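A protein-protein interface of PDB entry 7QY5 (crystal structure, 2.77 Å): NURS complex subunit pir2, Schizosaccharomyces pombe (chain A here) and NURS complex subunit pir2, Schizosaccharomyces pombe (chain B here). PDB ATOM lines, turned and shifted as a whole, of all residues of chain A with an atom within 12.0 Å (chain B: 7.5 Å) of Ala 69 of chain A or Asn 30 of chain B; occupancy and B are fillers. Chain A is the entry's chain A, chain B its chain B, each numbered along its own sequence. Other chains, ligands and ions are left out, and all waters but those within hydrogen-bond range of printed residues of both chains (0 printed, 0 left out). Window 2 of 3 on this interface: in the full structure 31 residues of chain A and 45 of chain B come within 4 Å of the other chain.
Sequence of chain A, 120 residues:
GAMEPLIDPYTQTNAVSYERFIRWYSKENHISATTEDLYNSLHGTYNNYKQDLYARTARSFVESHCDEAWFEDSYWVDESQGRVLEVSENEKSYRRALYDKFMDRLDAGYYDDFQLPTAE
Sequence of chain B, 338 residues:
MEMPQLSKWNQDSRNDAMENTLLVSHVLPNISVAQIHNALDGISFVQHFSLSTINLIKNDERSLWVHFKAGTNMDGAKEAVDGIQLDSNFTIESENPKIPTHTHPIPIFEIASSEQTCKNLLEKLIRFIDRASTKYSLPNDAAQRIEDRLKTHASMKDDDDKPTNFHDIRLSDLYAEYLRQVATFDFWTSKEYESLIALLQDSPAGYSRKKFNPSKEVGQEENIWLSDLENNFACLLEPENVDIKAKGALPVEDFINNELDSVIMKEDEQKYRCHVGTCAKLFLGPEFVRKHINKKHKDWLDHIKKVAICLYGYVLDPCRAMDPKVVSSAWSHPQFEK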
ATOM      1  N   PHE A  61      13.849  27.852  -6.099  1.00  0.00           N
ATOM      2  CA  PHE A  61      12.650  27.241  -6.736  1.00  0.00           C
ATOM      3  C   PHE A  61      13.068  26.556  -8.039  1.00  0.00           C
ATOM      4  O   PHE A  61      12.821  25.356  -8.208  1.00  0.00           O
ATOM      5  CB  PHE A  61      11.552  28.274  -7.019  1.00  0.00           C
ATOM      6  CG  PHE A  61      10.243  27.678  -7.487  1.00  0.00           C
ATOM      7  CD1 PHE A  61       9.921  27.634  -8.837  1.00  0.00           C
ATOM      8  CD2 PHE A  61       9.332  27.139  -6.585  1.00  0.00           C
ATOM      9  CE1 PHE A  61       8.724  27.080  -9.272  1.00  0.00           C
ATOM     10  CE2 PHE A  61       8.134  26.590  -7.022  1.00  0.00           C
ATOM     11  CZ  PHE A  61       7.833  26.556  -8.364  1.00  0.00           C
ATOM     12  N   VAL A  62      13.707  27.302  -8.935  1.00  0.00           N
ATOM     13  CA  VAL A  62      14.154  26.787 -10.263  1.00  0.00           C
ATOM     14  C   VAL A  62      15.022  25.533 -10.054  1.00  0.00           C
ATOM     15  O   VAL A  62      14.864  24.572 -10.823  1.00  0.00           O
ATOM     16  CB  VAL A  62      14.914  27.870 -11.051  1.00  0.00           C
ATOM     17  CG1 VAL A  62      15.509  27.318 -12.336  1.00  0.00           C
ATOM     18  CG2 VAL A  62      14.043  29.076 -11.347  1.00  0.00           C
ATOM     19  N   GLU A  63      15.909  25.540  -9.054  1.00  0.00           N
ATOM     20  CA  GLU A  63      16.925  24.471  -8.858  1.00  0.00           C
ATOM     21  C   GLU A  63      16.221  23.168  -8.517  1.00  0.00           C
ATOM     22  O   GLU A  63      16.679  22.125  -9.002  1.00  0.00           O
ATOM     23  CB  GLU A  63      17.930  24.799  -7.752  1.00  0.00           C
ATOM     24  CG  GLU A  63      19.360  24.945  -8.255  1.00  0.00           C
ATOM     25  CD  GLU A  63      20.210  25.886  -7.421  1.00  0.00           C
ATOM     26  OE1 GLU A  63      21.178  26.438  -7.983  1.00  0.00           O
ATOM     27  OE2 GLU A  63      19.892  26.088  -6.218  1.00  0.00           O
ATOM     28  N   SER A  64      15.168  23.235  -7.707  1.00  0.00           N
ATOM     29  CA  SER A  64      14.502  22.035  -7.143  1.00  0.00           C
ATOM     30  C   SER A  64      13.510  21.453  -8.155  1.00  0.00           C
ATOM     31  O   SER A  64      13.227  20.253  -8.064  1.00  0.00           O
ATOM     32  CB  SER A  64      13.845  22.349  -5.837  1.00  0.00           C
ATOM     33  OG  SER A  64      12.777  23.250  -6.039  1.00  0.00           O
ATOM     34  N   HIS A  65      13.006  22.261  -9.085  1.00  0.00           N
ATOM     35  CA  HIS A  65      11.915  21.853 -10.009  1.00  0.00           C
ATOM     36  C   HIS A  65      12.469  21.669 -11.427  1.00  0.00           C
ATOM     37  O   HIS A  65      11.722  21.150 -12.264  1.00  0.00           O
ATOM     38  CB  HIS A  65      10.738  22.855  -9.950  1.00  0.00           C
ATOM     39  CG  HIS A  65       9.892  22.771  -8.714  1.00  0.00           C
ATOM     40  ND1 HIS A  65       9.889  23.755  -7.745  1.00  0.00           N
ATOM     41  CD2 HIS A  65       9.019  21.834  -8.283  1.00  0.00           C
ATOM     42  CE1 HIS A  65       9.069  23.420  -6.768  1.00  0.00           C
ATOM     43  NE2 HIS A  65       8.519  22.253  -7.078  1.00  0.00           N
ATOM     44  N   CYS A  66      13.729  22.039 -11.680  1.00  0.00           N
ATOM     45  CA  CYS A  66      14.288  22.199 -13.057  1.00  0.00           C
ATOM     46  C   CYS A  66      14.119  20.916 -13.887  1.00  0.00           C
ATOM     47  O   CYS A  66      13.966  21.040 -15.127  1.00  0.00           O
ATOM     48  CB  CYS A  66      15.757  22.621 -13.053  1.00  0.00           C
ATOM     49  SG  CYS A  66      16.849  21.516 -12.125  1.00  0.00           S
ATOM     50  N   ASP A  67      14.137  19.742 -13.245  1.00  0.00           N
ATOM     51  CA  ASP A  67      14.161  18.424 -13.934  1.00  0.00           C
ATOM     52  C   ASP A  67      12.743  17.825 -14.041  1.00  0.00           C
ATOM     53  O   ASP A  67      12.589  16.762 -14.685  1.00  0.00           O
ATOM     54  CB  ASP A  67      15.161  17.510 -13.229  1.00  0.00           C
ATOM     55  CG  ASP A  67      16.600  17.842 -13.573  1.00  0.00           C
ATOM     56  OD1 ASP A  67      16.813  18.779 -14.384  1.00  0.00           O
ATOM     57  OD2 ASP A  67      17.495  17.145 -13.046  1.00  0.00           O
ATOM     58  N   GLU A  68      11.732  18.480 -13.464  1.00  0.00           N
ATOM     59  CA  GLU A  68      10.312  18.073 -13.605  1.00  0.00           C
ATOM     60  C   GLU A  68       9.885  18.368 -15.053  1.00  0.00           C
ATOM     61  O   GLU A  68      10.460  19.304 -15.677  1.00  0.00           O
ATOM     62  CB  GLU A  68       9.492  18.755 -12.512  1.00  0.00           C
ATOM     63  CG  GLU A  68      10.076  18.541 -11.127  1.00  0.00           C
ATOM     64  CD  GLU A  68       9.126  18.743  -9.956  1.00  0.00           C
ATOM     65  OE1 GLU A  68       9.542  18.546  -8.791  1.00  0.00           O
ATOM     66  OE2 GLU A  68       7.966  19.095 -10.197  1.00  0.00           O
ATOM     67  N   ALA A  69       8.968  17.562 -15.600  1.00  0.00           N
ATOM     68  CA  ALA A  69       8.617  17.531 -17.045  1.00  0.00           C
ATOM     69  C   ALA A  69       7.928  18.835 -17.445  1.00  0.00           C
ATOM     70  O   ALA A  69       8.258  19.370 -18.530  1.00  0.00           O
ATOM     71  CB  ALA A  69       7.734  16.350 -17.355  1.00  0.00           C
ATOM     72  N   TRP A  70       7.008  19.303 -16.592  1.00  0.00           N
ATOM     73  CA  TRP A  70       6.201  20.534 -16.802  1.00  0.00           C
ATOM     74  C   TRP A  70       7.114  21.757 -16.861  1.00  0.00           C
ATOM     75  O   TRP A  70       7.063  22.495 -17.881  1.00  0.00           O
ATOM     76  CB  TRP A  70       5.118  20.686 -15.729  1.00  0.00           C
ATOM     77  CG  TRP A  70       5.576  20.874 -14.316  1.00  0.00           C
ATOM     78  CD1 TRP A  70       5.644  19.913 -13.353  1.00  0.00           C
ATOM     79  CD2 TRP A  70       5.945  22.106 -13.671  1.00  0.00           C
ATOM     80  NE1 TRP A  70       6.053  20.455 -12.164  1.00  0.00           N
ATOM     81  CE2 TRP A  70       6.251  21.798 -12.327  1.00  0.00           C
ATOM     82  CE3 TRP A  70       6.055  23.435 -14.091  1.00  0.00           C
ATOM     83  CZ2 TRP A  70       6.662  22.766 -11.413  1.00  0.00           C
ATOM     84  CZ3 TRP A  70       6.454  24.394 -13.185  1.00  0.00           C
ATOM     85  CH2 TRP A  70       6.753  24.062 -11.866  1.00  0.00           C
ATOM     86  N   PHE A  71       7.948  21.932 -15.833  1.00  0.00           N
ATOM     87  CA  PHE A  71       8.862  23.091 -15.687  1.00  0.00           C
ATOM     88  C   PHE A  71       9.748  23.192 -16.931  1.00  0.00           C
ATOM     89  O   PHE A  71       9.793  24.279 -17.525  1.00  0.00           O
ATOM     90  CB  PHE A  71       9.665  22.983 -14.392  1.00  0.00           C
ATOM     91  CG  PHE A  71      10.471  24.221 -14.110  1.00  0.00           C
ATOM     92  CD1 PHE A  71      11.747  24.356 -14.625  1.00  0.00           C
ATOM     93  CD2 PHE A  71       9.933  25.270 -13.384  1.00  0.00           C
ATOM     94  CE1 PHE A  71      12.487  25.505 -14.398  1.00  0.00           C
ATOM     95  CE2 PHE A  71      10.678  26.412 -13.142  1.00  0.00           C
ATOM     96  CZ  PHE A  71      11.954  26.528 -13.653  1.00  0.00           C
ATOM     97  N   GLU A  72      10.385  22.088 -17.333  1.00  0.00           N
ATOM     98  CA  GLU A  72      11.179  21.994 -18.591  1.00  0.00           C
ATOM     99  C   GLU A  72      10.352  22.493 -19.790  1.00  0.00           C
ATOM    100  O   GLU A  72      10.915  23.283 -20.603  1.00  0.00           O
ATOM    101  CB  GLU A  72      11.629  20.553 -18.824  1.00  0.00           C
ATOM    102  CG  GLU A  72      12.661  20.047 -17.833  1.00  0.00           C
ATOM    103  CD  GLU A  72      12.954  18.557 -17.942  1.00  0.00           C
ATOM    104  OE1 GLU A  72      14.078  18.154 -17.597  1.00  0.00           O
ATOM    105  OE2 GLU A  72      12.053  17.799 -18.369  1.00  0.00           O
ATOM    106  N   ASP A  73       9.086  22.043 -19.897  1.00  0.00           N
ATOM    107  CA  ASP A  73       8.138  22.335 -21.014  1.00  0.00           C
ATOM    108  C   ASP A  73       7.790  23.832 -21.031  1.00  0.00           C
ATOM    109  O   ASP A  73       7.664  24.401 -22.152  1.00  0.00           O
ATOM    110  CB  ASP A  73       6.856  21.501 -20.912  1.00  0.00           C
ATOM    111  CG  ASP A  73       6.994  20.037 -21.304  1.00  0.00           C
ATOM    112  OD1 ASP A  73       7.840  19.741 -22.174  1.00  0.00           O
ATOM    113  OD2 ASP A  73       6.236  19.201 -20.745  1.00  0.00           O
ATOM    114  N   SER A  74       7.644  24.437 -19.844  1.00  0.00           N
ATOM    115  CA  SER A  74       7.359  25.884 -19.637  1.00  0.00           C
ATOM    116  C   SER A  74       8.535  26.772 -20.058  1.00  0.00           C
ATOM    117  O   SER A  74       8.314  27.723 -20.821  1.00  0.00           O
ATOM    118  CB  SER A  74       7.016  26.152 -18.211  1.00  0.00           C
ATOM    119  OG  SER A  74       5.688  25.767 -17.953  1.00  0.00           O
ATOM    120  N   TYR A  75       9.729  26.514 -19.535  1.00  0.00           N
ATOM    121  CA  TYR A  75      10.811  27.520 -19.459  1.00  0.00           C
ATOM    122  C   TYR A  75      12.093  27.065 -20.161  1.00  0.00           C
ATOM    123  O   TYR A  75      12.838  27.968 -20.606  1.00  0.00           O
ATOM    124  CB  TYR A  75      11.082  27.824 -17.990  1.00  0.00           C
ATOM    125  CG  TYR A  75       9.906  28.422 -17.261  1.00  0.00           C
ATOM    126  CD1 TYR A  75       9.414  29.660 -17.629  1.00  0.00           C
ATOM    127  CD2 TYR A  75       9.296  27.770 -16.199  1.00  0.00           C
ATOM    128  CE1 TYR A  75       8.345  30.238 -16.967  1.00  0.00           C
ATOM    129  CE2 TYR A  75       8.221  28.335 -15.530  1.00  0.00           C
ATOM    130  CZ  TYR A  75       7.745  29.577 -15.916  1.00  0.00           C
ATOM    131  OH  TYR A  75       6.688  30.183 -15.300  1.00  0.00           O
ATOM    132  N   TRP A  76      12.366  25.754 -20.236  1.00  0.00           N
ATOM    133  CA  TRP A  76      13.662  25.236 -20.757  1.00  0.00           C
ATOM    134  C   TRP A  76      13.698  25.317 -22.286  1.00  0.00           C
ATOM    135  O   TRP A  76      12.965  24.572 -22.940  1.00  0.00           O
ATOM    136  CB  TRP A  76      13.973  23.816 -20.276  1.00  0.00           C
ATOM    137  CG  TRP A  76      15.349  23.351 -20.660  1.00  0.00           C
ATOM    138  CD1 TRP A  76      16.459  24.118 -20.895  1.00  0.00           C
ATOM    139  CD2 TRP A  76      15.770  21.986 -20.841  1.00  0.00           C
ATOM    140  NE1 TRP A  76      17.529  23.328 -21.220  1.00  0.00           N
ATOM    141  CE2 TRP A  76      17.139  22.017 -21.188  1.00  0.00           C
ATOM    142  CE3 TRP A  76      15.121  20.749 -20.741  1.00  0.00           C
ATOM    143  CZ2 TRP A  76      17.866  20.854 -21.429  1.00  0.00           C
ATOM    144  CZ3 TRP A  76      15.842  19.603 -20.984  1.00  0.00           C
ATOM    145  CH2 TRP A  76      17.195  19.657 -21.324  1.00  0.00           C
ATOM    146  N   VAL A  77      14.589  26.163 -22.799  1.00  0.00           N
ATOM    147  CA  VAL A  77      14.808  26.447 -24.243  1.00  0.00           C
ATOM    148  C   VAL A  77      16.312  26.370 -24.524  1.00  0.00           C
ATOM    149  O   VAL A  77      17.080  26.911 -23.716  1.00  0.00           O
ATOM    150  CB  VAL A  77      14.244  27.834 -24.574  1.00  0.00           C
ATOM    151  CG1 VAL A  77      14.716  28.333 -25.931  1.00  0.00           C
ATOM    152  CG2 VAL A  77      12.727  27.831 -24.470  1.00  0.00           C
ATOM    153  N   GLY A  82      17.932  20.364 -28.456  1.00  0.00           N
ATOM    154  CA  GLY A  82      16.669  20.024 -29.149  1.00  0.00           C
ATOM    155  C   GLY A  82      15.434  20.429 -28.365  1.00  0.00           C
ATOM    156  O   GLY A  82      14.459  19.646 -28.354  1.00  0.00           O
ATOM    157  N   ARG A  83      15.482  21.608 -27.733  1.00  0.00           N
ATOM    158  CA  ARG A  83      14.390  22.210 -26.920  1.00  0.00           C
ATOM    159  C   ARG A  83      14.112  23.607 -27.487  1.00  0.00           C
ATOM    160  O   ARG A  83      15.082  24.337 -27.796  1.00  0.00           O
ATOM    161  CB  ARG A  83      14.774  22.231 -25.433  1.00  0.00           C
ATOM    162  CG  ARG A  83      14.456  20.945 -24.682  1.00  0.00           C
ATOM    163  CD  ARG A  83      13.144  21.040 -23.929  1.00  0.00           C
ATOM    164  NE  ARG A  83      12.881  19.847 -23.136  1.00  0.00           N
ATOM    165  CZ  ARG A  83      11.743  19.594 -22.490  1.00  0.00           C
ATOM    166  NH1 ARG A  83      10.739  20.455 -22.533  1.00  0.00           N
ATOM    167  NH2 ARG A  83      11.609  18.474 -21.798  1.00  0.00           N
ATOM    168  N   VAL A  84      12.834  23.932 -27.686  1.00  0.00           N
ATOM    169  CA  VAL A  84      12.357  25.277 -28.129  1.00  0.00           C
ATOM    170  C   VAL A  84      10.850  25.368 -27.825  1.00  0.00           C
ATOM    171  O   VAL A  84      10.271  24.350 -27.371  1.00  0.00           O
ATOM    172  CB  VAL A  84      12.710  25.542 -29.610  1.00  0.00           C
ATOM    173  CG1 VAL A  84      11.712  24.914 -30.570  1.00  0.00           C
ATOM    174  CG2 VAL A  84      12.881  27.030 -29.899  1.00  0.00           C
ATOM    175  N   LEU A  85      10.258  26.556 -27.968  1.00  0.00           N
ATOM    176  CA  LEU A  85       8.803  26.796 -27.787  1.00  0.00           C
ATOM    177  C   LEU A  85       8.310  27.577 -29.005  1.00  0.00           C
ATOM    178  O   LEU A  85       8.756  28.728 -29.173  1.00  0.00           O
ATOM    179  CB  LEU A  85       8.576  27.561 -26.477  1.00  0.00           C
ATOM    180  CG  LEU A  85       9.018  26.835 -25.203  1.00  0.00           C
ATOM    181  CD1 LEU A  85       9.017  27.769 -24.001  1.00  0.00           C
ATOM    182  CD2 LEU A  85       8.142  25.622 -24.927  1.00  0.00           C
ATOM    183  N   VAL B  27      -3.500  15.093 -13.701  1.00  0.00           N
ATOM    184  CA  VAL B  27      -2.325  15.045 -14.613  1.00  0.00           C
ATOM    185  C   VAL B  27      -1.045  15.277 -13.799  1.00  0.00           C
ATOM    186  O   VAL B  27      -0.871  16.370 -13.225  1.00  0.00           O
ATOM    187  CB  VAL B  27      -2.475  16.061 -15.754  1.00  0.00           C
ATOM    188  CG1 VAL B  27      -1.322  15.957 -16.738  1.00  0.00           C
ATOM    189  CG2 VAL B  27      -3.807  15.885 -16.459  1.00  0.00           C
ATOM    190  N   LEU B  28      -0.168  14.277 -13.778  1.00  0.00           N
ATOM    191  CA  LEU B  28       1.047  14.259 -12.926  1.00  0.00           C
ATOM    192  C   LEU B  28       2.134  15.138 -13.541  1.00  0.00           C
ATOM    193  O   LEU B  28       2.226  15.265 -14.759  1.00  0.00           O
ATOM    194  CB  LEU B  28       1.553  12.820 -12.766  1.00  0.00           C
ATOM    195  CG  LEU B  28       0.564  11.788 -12.216  1.00  0.00           C
ATOM    196  CD1 LEU B  28       1.274  10.468 -11.961  1.00  0.00           C
ATOM    197  CD2 LEU B  28      -0.127  12.263 -10.946  1.00  0.00           C
ATOM    198  N   PRO B  29       2.998  15.725 -12.681  1.00  0.00           N
ATOM    199  CA  PRO B  29       4.088  16.613 -13.107  1.00  0.00           C
ATOM    200  C   PRO B  29       5.138  16.077 -14.099  1.00  0.00           C
ATOM    201  O   PRO B  29       5.643  16.824 -14.921  1.00  0.00           O
ATOM    202  CB  PRO B  29       4.845  16.853 -11.790  1.00  0.00           C
ATOM    203  CG  PRO B  29       3.813  16.659 -10.692  1.00  0.00           C
ATOM    204  CD  PRO B  29       2.914  15.572 -11.216  1.00  0.00           C
ATOM    205  N   ASN B  30       5.483  14.802 -13.949  1.00  0.00           N
ATOM    206  CA  ASN B  30       6.507  14.070 -14.743  1.00  0.00           C
ATOM    207  C   ASN B  30       6.032  13.901 -16.188  1.00  0.00           C
ATOM    208  O   ASN B  30       6.870  13.561 -17.028  1.00  0.00           O
ATOM    209  CB  ASN B  30       6.781  12.690 -14.136  1.00  0.00           C
ATOM    210  CG  ASN B  30       5.512  11.912 -13.813  1.00  0.00           C
ATOM    211  OD1 ASN B  30       4.583  11.866 -14.617  1.00  0.00           O
ATOM    212  ND2 ASN B  30       5.443  11.310 -12.633  1.00  0.00           N
ATOM    213  N   ILE B  31       4.732  14.070 -16.445  1.00  0.00           N
ATOM    214  CA  ILE B  31       4.117  13.893 -17.793  1.00  0.00           C
ATOM    215  C   ILE B  31       4.541  15.058 -18.679  1.00  0.00           C
ATOM    216  O   ILE B  31       4.148  16.200 -18.378  1.00  0.00           O
ATOM    217  CB  ILE B  31       2.589  13.811 -17.703  1.00  0.00           C
ATOM    218  CG1 ILE B  31       2.151  12.530 -16.988  1.00  0.00           C
ATOM    219  CG2 ILE B  31       1.983  13.949 -19.090  1.00  0.00           C
ATOM    220  CD1 ILE B  31       0.679  12.470 -16.670  1.00  0.00           C
ATOM    221  N   SER B  32       5.308  14.778 -19.728  1.00  0.00           N
ATOM    222  CA  SER B  32       5.859  15.819 -20.625  1.00  0.00           C
ATOM    223  C   SER B  32       4.791  16.180 -21.651  1.00  0.00           C
ATOM    224  O   SER B  32       3.770  15.494 -21.718  1.00  0.00           O
ATOM    225  CB  SER B  32       7.149  15.378 -21.265  1.00  0.00           C
ATOM    226  OG  SER B  32       6.910  14.590 -22.416  1.00  0.00           O
ATOM    227  N   VAL B  33       5.022  17.258 -22.385  1.00  0.00           N
ATOM    228  CA  VAL B  33       4.149  17.724 -23.502  1.00  0.00           C
ATOM    229  C   VAL B  33       4.407  16.776 -24.680  1.00  0.00           C
ATOM    230  O   VAL B  33       3.426  16.280 -25.258  1.00  0.00           O
ATOM    231  CB  VAL B  33       4.418  19.215 -23.818  1.00  0.00           C
ATOM    232  CG1 VAL B  33       4.014  19.621 -25.222  1.00  0.00           C
ATOM    233  CG2 VAL B  33       3.753  20.129 -22.803  1.00  0.00           C
ATOM    234  N   GLN B  35       5.170  13.696 -24.827  1.00  0.00           N
ATOM    235  CA  GLN B  35       4.339  12.493 -24.566  1.00  0.00           C
ATOM    236  C   GLN B  35       2.909  12.708 -25.085  1.00  0.00           C
ATOM    237  O   GLN B  35       2.381  11.814 -25.803  1.00  0.00           O
ATOM    238  CB  GLN B  35       4.285  12.207 -23.068  1.00  0.00           C
ATOM    239  CG  GLN B  35       5.576  11.654 -22.494  1.00  0.00           C
ATOM    240  CD  GLN B  35       5.378  11.357 -21.028  1.00  0.00           C
ATOM    241  OE1 GLN B  35       4.631  12.048 -20.336  1.00  0.00           O
ATOM    242  NE2 GLN B  35       6.031  10.315 -20.539  1.00  0.00           N
ATOM    243  N   ASP B  60      -0.337  19.041  -6.693  1.00  0.00           N
ATOM    244  CA  ASP B  60       0.781  18.800  -7.647  1.00  0.00           C
ATOM    245  C   ASP B  60       0.241  18.398  -9.036  1.00  0.00           C
ATOM    246  O   ASP B  60       1.066  18.104  -9.945  1.00  0.00           O
ATOM    247  CB  ASP B  60       1.738  17.785  -7.020  1.00  0.00           C
ATOM    248  CG  ASP B  60       2.169  18.177  -5.609  1.00  0.00           C
ATOM    249  OD1 ASP B  60       2.849  17.367  -4.953  1.00  0.00           O
ATOM    250  OD2 ASP B  60       1.819  19.300  -5.171  1.00  0.00           O
ATOM    251  N   ARG B  62      -2.022  19.125 -12.541  1.00  0.00           N
ATOM    252  CA  ARG B  62      -2.659  20.008 -13.550  1.00  0.00           C
ATOM    253  C   ARG B  62      -3.954  19.339 -14.046  1.00  0.00           C
ATOM    254  O   ARG B  62      -4.414  18.346 -13.423  1.00  0.00           O
ATOM    255  CB  ARG B  62      -1.680  20.305 -14.694  1.00  0.00           C
ATOM    256  CG  ARG B  62      -0.262  20.637 -14.246  1.00  0.00           C
ATOM    257  CD  ARG B  62       0.752  19.579 -14.646  1.00  0.00           C
ATOM    258  NE  ARG B  62       1.319  19.824 -15.974  1.00  0.00           N
ATOM    259  CZ  ARG B  62       2.156  18.998 -16.621  1.00  0.00           C
ATOM    260  NH1 ARG B  62       2.532  17.852 -16.071  1.00  0.00           N
ATOM    261  NH2 ARG B  62       2.624  19.311 -17.820  1.00  0.00           N
ATOM    262  N   ASP B  87       2.468   7.510 -19.894  1.00  0.00           N
ATOM    263  CA  ASP B  87       3.622   6.790 -19.305  1.00  0.00           C
ATOM    264  C   ASP B  87       3.074   5.650 -18.439  1.00  0.00           C
ATOM    265  O   ASP B  87       1.840   5.558 -18.303  1.00  0.00           O
ATOM    266  CB  ASP B  87       4.521   7.755 -18.530  1.00  0.00           C
ATOM    267  CG  ASP B  87       5.885   7.171 -18.199  1.00  0.00           C
ATOM    268  OD1 ASP B  87       6.185   6.048 -18.680  1.00  0.00           O
ATOM    269  OD2 ASP B  87       6.632   7.831 -17.455  1.00  0.00           O
ATOM    270  N   ASN B  89       2.912   5.449 -15.312  1.00  0.00           N
ATOM    271  CA  ASN B  89       2.277   5.949 -14.059  1.00  0.00           C
ATOM    272  C   ASN B  89       0.902   6.600 -14.301  1.00  0.00           C
ATOM    273  O   ASN B  89       0.167   6.741 -13.301  1.00  0.00           O
ATOM    274  CB  ASN B  89       3.181   6.931 -13.306  1.00  0.00           C
ATOM    275  CG  ASN B  89       3.865   7.939 -14.204  1.00  0.00           C
ATOM    276  OD1 ASN B  89       3.409   8.216 -15.317  1.00  0.00           O
ATOM    277  ND2 ASN B  89       4.978   8.479 -13.736  1.00  0.00           N
ATOM    278  N   PHE B  90       0.561   7.024 -15.531  1.00  0.00           N
ATOM    279  CA  PHE B  90      -0.727   7.715 -15.844  1.00  0.00           C
ATOM    280  C   PHE B  90      -1.284   7.278 -17.202  1.00  0.00           C
ATOM    281  O   PHE B  90      -0.684   7.563 -18.264  1.00  0.00           O
ATOM    282  CB  PHE B  90      -0.580   9.239 -15.822  1.00  0.00           C
ATOM    283  CG  PHE B  90      -1.883   9.999 -15.809  1.00  0.00           C
ATOM    284  CD1 PHE B  90      -2.256  10.784 -16.888  1.00  0.00           C
ATOM    285  CD2 PHE B  90      -2.735   9.942 -14.712  1.00  0.00           C
ATOM    286  CE1 PHE B  90      -3.452  11.489 -16.870  1.00  0.00           C
ATOM    287  CE2 PHE B  90      -3.934  10.642 -14.699  1.00  0.00           C
ATOM    288  CZ  PHE B  90      -4.291  11.415 -15.781  1.00  0.00           C
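Of the 21 printed residues of chain A, 3 touch a printed residue of chain B. Among the printed residues, no Asp or Glu carboxylate lies within 4 Å of a Lys or Arg side-chain nitrogen of the other chain.
Ala 69 of chain A touches four residues of chain B. Printed residues of chain B within 4 Å of Trp 70 of chain A: Pro 29 (3.3 Å) and Arg 62 (3.5 Å). Of the printed residues of chain B, Asp 73 of chain A touches Ser 32 and Val 33. Val 84 of chain A touches none of the printed residues of chain B. No residue of chain A comes within 4 Å of Leu 28 of chain B. Of chain A, only Ala 69 comes within 4 Å of Asn 30 of chain B. Of chain A, only Ala 69 (3.7 Å) comes within 4 Å of Ile 31 of chain B. Of chain A, only Ala 69 and Asp 73 come within 4 Å of Ser 32 of chain B. Of the printed residues of chain A, Val 33 of chain B touches Asp 73. No residue of chain A comes within 4 Å of Asn 89 of chain B. Phe 90 of chain B touches none of the printed residues of chain A. The nearest residue of chain A that does not touch Asn 30 of chain B is Trp 70 of chain A (5.1 Å).
N of Ala 69 of chain A sits close to O of Pro 29 of chain B. O of Pro 29 of chain B is in hydrogen-bond range of N of Trp 70 of chain A. N of Val 33 of chain B sits at hydrogen-bond distance from OD2 of Asp 73 of chain A (2.8 Å).
The side-chain carboxylate (OE2) of Glu 68 of chain A is in hydrogen-bond range of the indole nitrogen (NE1) of Trp 70 of chain A (3.1 Å). OD1 of Asp 73 of chain A lies within salt-bridge range of NH1 of Arg 83 of chain A. O of Leu 28 of chain B sits at hydrogen-bond distance from NH1 of Arg 62 of chain B, 2.9 Å away. The backbone carbonyl oxygen (O) of Pro 29 of chain B sits at hydrogen-bond distance from the guanidinium group (NH1) of Arg 62 of chain B (3.5 Å). The guanidinium group of Arg 62 of chain B lies within hydrogen-bond range of the backbone carbonyl oxygen of Ile 31 of chain B (3.3 Å). The side-chain amide oxygen (OE1) of Gln 35 of chain B sits at hydrogen-bond distance from the backbone NH (N) of Ser 32 of chain B (2.9 Å).
Among the printed residues, pairs that only touch across the chains: Ala 69 of chain A with Asn 30 of chain B (2.9 Å), Asp 73 of chain A with Ser 32 of chain B (3.4 Å), Trp 70 of chain A with Arg 62 of chain B (3.5 Å), Ala 69 of chain A with Ile 31 of chain B (3.7 Å) and Ala 69 of chain A with Ser 32 of chain B (3.7 Å).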
